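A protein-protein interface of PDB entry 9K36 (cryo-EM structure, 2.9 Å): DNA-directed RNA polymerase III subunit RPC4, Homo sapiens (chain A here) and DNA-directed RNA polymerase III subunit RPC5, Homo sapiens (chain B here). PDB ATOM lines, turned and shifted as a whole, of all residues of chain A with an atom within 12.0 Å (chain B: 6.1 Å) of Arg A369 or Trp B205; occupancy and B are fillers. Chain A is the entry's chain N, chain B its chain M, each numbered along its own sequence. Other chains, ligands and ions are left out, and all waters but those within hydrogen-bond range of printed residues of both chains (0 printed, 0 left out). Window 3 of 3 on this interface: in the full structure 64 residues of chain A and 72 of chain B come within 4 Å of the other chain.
Hydrophobic or aromatic side chains of chain A within 4 Å of the printed part of chain B: Val A363 and Met A373.
Among the printed residues, 6 pairs touch across the chains.
Among the printed residues, no Asp or Glu carboxylate lies within 4 Å of a Lys or Arg side-chain nitrogen of the other chain.
The backbone carbonyl oxygen of Ile B49 sits at hydrogen-bond distance from the backbone NH of Val B206 (2.9 Å).
Arg A369 touches just these residues of chain B: Trp B205 (3.3 Å), Val B206 (3.4 Å) and His B207 (3.5 Å).
Trp B205 touches just one residue of chain A: Arg A369.
No residue of chain A comes within 4 Å of Ile B49.
No residue of chain A comes within 4 Å of Lys B50.
No residue of chain A comes within 4 Å of Val B56.
No residue of chain A comes within 4 Å of Glu B57.
No residue of chain A comes within 4 Å of Glu B203.
Val B206 touches one residue of chain A.
Of chain A, only Arg A369 (3.5 Å) comes within 4 Å of His B207.
Of the printed residues of chain B, Gly A371 touches Leu B208 (3.4 Å).
Printed residues of chain B within 4 Å of Val A363: Leu B208.
Of the printed residues of chain A, Leu B208 touches Val A363, Gly A371 and Met A373.
Ser A368 touches none of the printed residues of chain B.
The nearest residue of chain A that does not touch Trp B205 is Ser A368 (7.1 Å).
NH2 of Arg A369 lies within hydrogen-bond range of O of Trp B205 (3.3 Å).
Among the printed residues, merely in contact across the chains: Val A363 with Leu B208, Arg A369 with Val B206, Arg A369 with His B207, Gly A371 with Leu B208 and Met A373 with Leu B208.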
ATOM      1  N   VAL A 363      -1.066  24.402  16.471  1.00  0.00           N
ATOM      2  CA  VAL A 363      -2.266  24.134  15.680  1.00  0.00           C
ATOM      3  C   VAL A 363      -3.449  24.301  16.628  1.00  0.00           C
ATOM      4  O   VAL A 363      -3.828  23.384  17.357  1.00  0.00           O
ATOM      5  CB  VAL A 363      -2.229  22.750  15.035  1.00  0.00           C
ATOM      6  CG1 VAL A 363      -3.487  22.519  14.206  1.00  0.00           C
ATOM      7  CG2 VAL A 363      -0.985  22.601  14.171  1.00  0.00           C
ATOM      8  N   GLY A 364      -4.046  25.492  16.611  1.00  0.00           N
ATOM      9  CA  GLY A 364      -5.162  25.790  17.486  1.00  0.00           C
ATOM     10  C   GLY A 364      -6.506  25.754  16.788  1.00  0.00           C
ATOM     11  O   GLY A 364      -6.802  26.610  15.949  1.00  0.00           O
ATOM     12  N   LEU A 365      -7.330  24.762  17.130  1.00  0.00           N
ATOM     13  CA  LEU A 365      -8.664  24.618  16.544  1.00  0.00           C
ATOM     14  C   LEU A 365      -9.642  25.466  17.350  1.00  0.00           C
ATOM     15  O   LEU A 365     -10.382  24.983  18.211  1.00  0.00           O
ATOM     16  CB  LEU A 365      -9.086  23.155  16.507  1.00  0.00           C
ATOM     17  CG  LEU A 365      -8.406  22.218  15.503  1.00  0.00           C
ATOM     18  CD1 LEU A 365      -7.032  21.773  15.986  1.00  0.00           C
ATOM     19  CD2 LEU A 365      -9.292  21.015  15.217  1.00  0.00           C
ATOM     20  N   GLY A 366      -9.639  26.769  17.060  1.00  0.00           N
ATOM     21  CA  GLY A 366     -10.537  27.675  17.757  1.00  0.00           C
ATOM     22  C   GLY A 366     -11.997  27.407  17.444  1.00  0.00           C
ATOM     23  O   GLY A 366     -12.860  27.506  18.319  1.00  0.00           O
ATOM     24  N   ASP A 367     -12.293  27.059  16.193  1.00  0.00           N
ATOM     25  CA  ASP A 367     -13.643  26.737  15.762  1.00  0.00           C
ATOM     26  C   ASP A 367     -13.690  25.292  15.283  1.00  0.00           C
ATOM     27  O   ASP A 367     -12.681  24.731  14.846  1.00  0.00           O
ATOM     28  CB  ASP A 367     -14.110  27.680  14.645  1.00  0.00           C
ATOM     29  CG  ASP A 367     -15.591  27.551  14.351  1.00  0.00           C
ATOM     30  OD1 ASP A 367     -16.286  26.832  15.100  1.00  0.00           O
ATOM     31  OD2 ASP A 367     -16.060  28.165  13.370  1.00  0.00           O
ATOM     32  N   SER A 368     -14.879  24.692  15.370  1.00  0.00           N
ATOM     33  CA  SER A 368     -15.063  23.313  14.933  1.00  0.00           C
ATOM     34  C   SER A 368     -14.961  23.150  13.421  1.00  0.00           C
ATOM     35  O   SER A 368     -14.893  22.013  12.944  1.00  0.00           O
ATOM     36  CB  SER A 368     -16.416  22.788  15.417  1.00  0.00           C
ATOM     37  OG  SER A 368     -16.620  21.446  15.010  1.00  0.00           O
ATOM     38  N   ARG A 369     -14.949  24.246  12.668  1.00  0.00           N
ATOM     39  CA  ARG A 369     -14.843  24.196  11.216  1.00  0.00           C
ATOM     40  C   ARG A 369     -13.564  24.818  10.677  1.00  0.00           C
ATOM     41  O   ARG A 369     -13.042  24.338   9.668  1.00  0.00           O
ATOM     42  CB  ARG A 369     -16.050  24.898  10.571  1.00  0.00           C
ATOM     43  CG  ARG A 369     -16.088  24.860   9.046  1.00  0.00           C
ATOM     44  CD  ARG A 369     -16.302  23.450   8.512  1.00  0.00           C
ATOM     45  NE  ARG A 369     -15.046  22.728   8.328  1.00  0.00           N
ATOM     46  CZ  ARG A 369     -14.961  21.479   7.881  1.00  0.00           C
ATOM     47  NH1 ARG A 369     -16.061  20.808   7.569  1.00  0.00           N
ATOM     48  NH2 ARG A 369     -13.776  20.901   7.745  1.00  0.00           N
ATOM     49  N   THR A 370     -13.036  25.855  11.325  1.00  0.00           N
ATOM     50  CA  THR A 370     -11.827  26.525  10.867  1.00  0.00           C
ATOM     51  C   THR A 370     -10.874  26.695  12.040  1.00  0.00           C
ATOM     52  O   THR A 370     -11.275  27.171  13.106  1.00  0.00           O
ATOM     53  CB  THR A 370     -12.149  27.890  10.245  1.00  0.00           C
ATOM     54  OG1 THR A 370     -13.037  27.713   9.136  1.00  0.00           O
ATOM     55  CG2 THR A 370     -10.878  28.575   9.768  1.00  0.00           C
ATOM     56  N   GLY A 371      -9.611  26.305  11.837  1.00  0.00           N
ATOM     57  CA  GLY A 371      -8.598  26.444  12.856  1.00  0.00           C
ATOM     58  C   GLY A 371      -7.404  27.220  12.327  1.00  0.00           C
ATOM     59  O   GLY A 371      -7.305  27.514  11.134  1.00  0.00           O
ATOM     60  N   GLU A 372      -6.495  27.546  13.242  1.00  0.00           N
ATOM     61  CA  GLU A 372      -5.310  28.331  12.931  1.00  0.00           C
ATOM     62  C   GLU A 372      -4.060  27.527  13.254  1.00  0.00           C
ATOM     63  O   GLU A 372      -3.964  26.923  14.328  1.00  0.00           O
ATOM     64  CB  GLU A 372      -5.302  29.648  13.710  1.00  0.00           C
ATOM     65  CG  GLU A 372      -6.501  30.540  13.436  1.00  0.00           C
ATOM     66  CD  GLU A 372      -6.460  31.831  14.229  1.00  0.00           C
ATOM     67  OE1 GLU A 372      -5.521  32.010  15.033  1.00  0.00           O
ATOM     68  OE2 GLU A 372      -7.369  32.671  14.048  1.00  0.00           O
ATOM     69  N   MET A 373      -3.106  27.523  12.327  1.00  0.00           N
ATOM     70  CA  MET A 373      -1.797  26.919  12.539  1.00  0.00           C
ATOM     71  C   MET A 373      -0.773  28.035  12.699  1.00  0.00           C
ATOM     72  O   MET A 373      -0.579  28.839  11.782  1.00  0.00           O
ATOM     73  CB  MET A 373      -1.416  26.002  11.378  1.00  0.00           C
ATOM     74  CG  MET A 373      -2.377  24.851  11.148  1.00  0.00           C
ATOM     75  SD  MET A 373      -1.772  23.728   9.874  1.00  0.00           S
ATOM     76  CE  MET A 373      -1.371  24.894   8.575  1.00  0.00           C
ATOM     77  N   LYS B  48      -5.110  19.707   5.506  1.00  0.00           N
ATOM     78  CA  LYS B  48      -6.134  18.794   5.986  1.00  0.00           C
ATOM     79  C   LYS B  48      -5.648  18.111   7.260  1.00  0.00           C
ATOM     80  O   LYS B  48      -4.466  17.798   7.402  1.00  0.00           O
ATOM     81  CB  LYS B  48      -6.475  17.752   4.919  1.00  0.00           C
ATOM     82  CG  LYS B  48      -6.875  18.354   3.579  1.00  0.00           C
ATOM     83  CD  LYS B  48      -7.125  17.278   2.534  1.00  0.00           C
ATOM     84  CE  LYS B  48      -8.280  16.378   2.934  1.00  0.00           C
ATOM     85  NZ  LYS B  48      -8.546  15.327   1.912  1.00  0.00           N
ATOM     86  N   ILE B  49      -6.570  17.895   8.197  1.00  0.00           N
ATOM     87  CA  ILE B  49      -6.205  17.327   9.490  1.00  0.00           C
ATOM     88  C   ILE B  49      -7.426  16.655  10.092  1.00  0.00           C
ATOM     89  O   ILE B  49      -8.567  16.978   9.748  1.00  0.00           O
ATOM     90  CB  ILE B  49      -5.624  18.415  10.432  1.00  0.00           C
ATOM     91  CG1 ILE B  49      -4.764  17.782  11.529  1.00  0.00           C
ATOM     92  CG2 ILE B  49      -6.741  19.241  11.047  1.00  0.00           C
ATOM     93  CD1 ILE B  49      -4.180  18.784  12.499  1.00  0.00           C
ATOM     94  N   LYS B  50      -7.182  15.702  10.992  1.00  0.00           N
ATOM     95  CA  LYS B  50      -8.230  15.026  11.748  1.00  0.00           C
ATOM     96  C   LYS B  50      -7.941  15.166  13.233  1.00  0.00           C
ATOM     97  O   LYS B  50      -6.787  14.968  13.650  1.00  0.00           O
ATOM     98  CB  LYS B  50      -8.318  13.550  11.361  1.00  0.00           C
ATOM     99  CG  LYS B  50      -8.683  13.304   9.909  1.00  0.00           C
ATOM    100  CD  LYS B  50      -8.766  11.818   9.610  1.00  0.00           C
ATOM    101  CE  LYS B  50      -9.205  11.575   8.175  1.00  0.00           C
ATOM    102  NZ  LYS B  50      -9.266  10.124   7.851  1.00  0.00           N
ATOM    103  N   LYS B  55      -3.400  12.862  11.445  1.00  0.00           N
ATOM    104  CA  LYS B  55      -2.616  12.677  10.224  1.00  0.00           C
ATOM    105  C   LYS B  55      -2.857  13.903   9.350  1.00  0.00           C
ATOM    106  O   LYS B  55      -3.882  13.985   8.663  1.00  0.00           O
ATOM    107  CB  LYS B  55      -3.000  11.389   9.508  1.00  0.00           C
ATOM    108  CG  LYS B  55      -2.163  11.092   8.274  1.00  0.00           C
ATOM    109  CD  LYS B  55      -2.503   9.730   7.693  1.00  0.00           C
ATOM    110  CE  LYS B  55      -3.943   9.675   7.209  1.00  0.00           C
ATOM    111  NZ  LYS B  55      -4.194  10.640   6.104  1.00  0.00           N
ATOM    112  N   VAL B  56      -1.920  14.842   9.377  1.00  0.00           N
ATOM    113  CA  VAL B  56      -2.066  16.112   8.672  1.00  0.00           C
ATOM    114  C   VAL B  56      -1.443  15.994   7.287  1.00  0.00           C
ATOM    115  O   VAL B  56      -0.379  15.392   7.109  1.00  0.00           O
ATOM    116  CB  VAL B  56      -1.436  17.265   9.481  1.00  0.00           C
ATOM    117  CG1 VAL B  56       0.037  17.000   9.755  1.00  0.00           C
ATOM    118  CG2 VAL B  56      -1.621  18.595   8.763  1.00  0.00           C
ATOM    119  N   GLU B  57      -2.128  16.559   6.295  1.00  0.00           N
ATOM    120  CA  GLU B  57      -1.660  16.602   4.914  1.00  0.00           C
ATOM    121  C   GLU B  57      -1.579  18.064   4.494  1.00  0.00           C
ATOM    122  O   GLU B  57      -2.607  18.744   4.395  1.00  0.00           O
ATOM    123  CB  GLU B  57      -2.586  15.812   3.990  1.00  0.00           C
ATOM    124  CG  GLU B  57      -2.140  15.793   2.539  1.00  0.00           C
ATOM    125  CD  GLU B  57      -3.054  14.966   1.656  1.00  0.00           C
ATOM    126  OE1 GLU B  57      -4.009  14.360   2.183  1.00  0.00           O
ATOM    127  OE2 GLU B  57      -2.813  14.920   0.432  1.00  0.00           O
ATOM    128  N   ALA B 201     -10.476   6.591   7.040  1.00  0.00           N
ATOM    129  CA  ALA B 201     -11.166   7.476   6.109  1.00  0.00           C
ATOM    130  C   ALA B 201     -12.580   7.817   6.560  1.00  0.00           C
ATOM    131  O   ALA B 201     -13.147   8.803   6.076  1.00  0.00           O
ATOM    132  CB  ALA B 201     -11.203   6.845   4.717  1.00  0.00           C
ATOM    133  N   GLU B 203     -13.474   9.038   9.336  1.00  0.00           N
ATOM    134  CA  GLU B 203     -13.450  10.303  10.058  1.00  0.00           C
ATOM    135  C   GLU B 203     -13.373  11.460   9.067  1.00  0.00           C
ATOM    136  O   GLU B 203     -12.515  11.452   8.175  1.00  0.00           O
ATOM    137  CB  GLU B 203     -12.267  10.345  11.022  1.00  0.00           C
ATOM    138  CG  GLU B 203     -12.199  11.599  11.876  1.00  0.00           C
ATOM    139  CD  GLU B 203     -11.159  11.499  12.972  1.00  0.00           C
ATOM    140  OE1 GLU B 203     -10.630  10.388  13.191  1.00  0.00           O
ATOM    141  OE2 GLU B 203     -10.868  12.531  13.615  1.00  0.00           O
ATOM    142  N   PRO B 204     -14.240  12.464   9.181  1.00  0.00           N
ATOM    143  CA  PRO B 204     -14.223  13.565   8.213  1.00  0.00           C
ATOM    144  C   PRO B 204     -12.985  14.435   8.361  1.00  0.00           C
ATOM    145  O   PRO B 204     -12.398  14.550   9.437  1.00  0.00           O
ATOM    146  CB  PRO B 204     -15.494  14.351   8.551  1.00  0.00           C
ATOM    147  CG  PRO B 204     -15.739  14.056   9.993  1.00  0.00           C
ATOM    148  CD  PRO B 204     -15.290  12.636  10.200  1.00  0.00           C
ATOM    149  N   TRP B 205     -12.592  15.051   7.250  1.00  0.00           N
ATOM    150  CA  TRP B 205     -11.424  15.916   7.228  1.00  0.00           C
ATOM    151  C   TRP B 205     -11.776  17.321   7.698  1.00  0.00           C
ATOM    152  O   TRP B 205     -12.926  17.763   7.610  1.00  0.00           O
ATOM    153  CB  TRP B 205     -10.826  15.982   5.821  1.00  0.00           C
ATOM    154  CG  TRP B 205     -10.121  14.729   5.400  1.00  0.00           C
ATOM    155  CD1 TRP B 205     -10.617  13.735   4.606  1.00  0.00           C
ATOM    156  CD2 TRP B 205      -8.788  14.336   5.748  1.00  0.00           C
ATOM    157  NE1 TRP B 205      -9.676  12.749   4.438  1.00  0.00           N
ATOM    158  CE2 TRP B 205      -8.544  13.093   5.130  1.00  0.00           C
ATOM    159  CE3 TRP B 205      -7.778  14.915   6.524  1.00  0.00           C
ATOM    160  CZ2 TRP B 205      -7.331  12.420   5.265  1.00  0.00           C
ATOM    161  CZ3 TRP B 205      -6.576  14.244   6.654  1.00  0.00           C
ATOM    162  CH2 TRP B 205      -6.362  13.010   6.029  1.00  0.00           C
ATOM    163  N   VAL B 206     -10.765  18.024   8.203  1.00  0.00           N
ATOM    164  CA  VAL B 206     -10.891  19.402   8.658  1.00  0.00           C
ATOM    165  C   VAL B 206      -9.846  20.236   7.930  1.00  0.00           C
ATOM    166  O   VAL B 206      -8.659  19.891   7.932  1.00  0.00           O
ATOM    167  CB  VAL B 206     -10.716  19.521  10.184  1.00  0.00           C
ATOM    168  CG1 VAL B 206     -10.825  20.974  10.621  1.00  0.00           C
ATOM    169  CG2 VAL B 206     -11.744  18.662  10.904  1.00  0.00           C
ATOM    170  N   HIS B 207     -10.290  21.325   7.308  1.00  0.00           N
ATOM    171  CA  HIS B 207      -9.406  22.200   6.550  1.00  0.00           C
ATOM    172  C   HIS B 207      -8.904  23.339   7.426  1.00  0.00           C
ATOM    173  O   HIS B 207      -9.662  23.918   8.210  1.00  0.00           O
ATOM    174  CB  HIS B 207     -10.127  22.767   5.325  1.00  0.00           C
ATOM    175  CG  HIS B 207     -10.513  21.731   4.316  1.00  0.00           C
ATOM    176  ND1 HIS B 207     -11.415  20.725   4.588  1.00  0.00           N
ATOM    177  CD2 HIS B 207     -10.122  21.546   3.033  1.00  0.00           C
ATOM    178  CE1 HIS B 207     -11.562  19.966   3.518  1.00  0.00           C
ATOM    179  NE2 HIS B 207     -10.788  20.444   2.558  1.00  0.00           N
ATOM    180  N   LEU B 208      -7.623  23.668   7.276  1.00  0.00           N
ATOM    181  CA  LEU B 208      -6.983  24.719   8.049  1.00  0.00           C
ATOM    182  C   LEU B 208      -6.127  25.574   7.127  1.00  0.00           C
ATOM    183  O   LEU B 208      -5.524  25.067   6.175  1.00  0.00           O
ATOM    184  CB  LEU B 208      -6.102  24.148   9.169  1.00  0.00           C
ATOM    185  CG  LEU B 208      -6.652  23.063  10.096  1.00  0.00           C
ATOM    186  CD1 LEU B 208      -5.575  22.642  11.081  1.00  0.00           C
ATOM    187  CD2 LEU B 208      -7.887  23.543  10.832  1.00  0.00           C
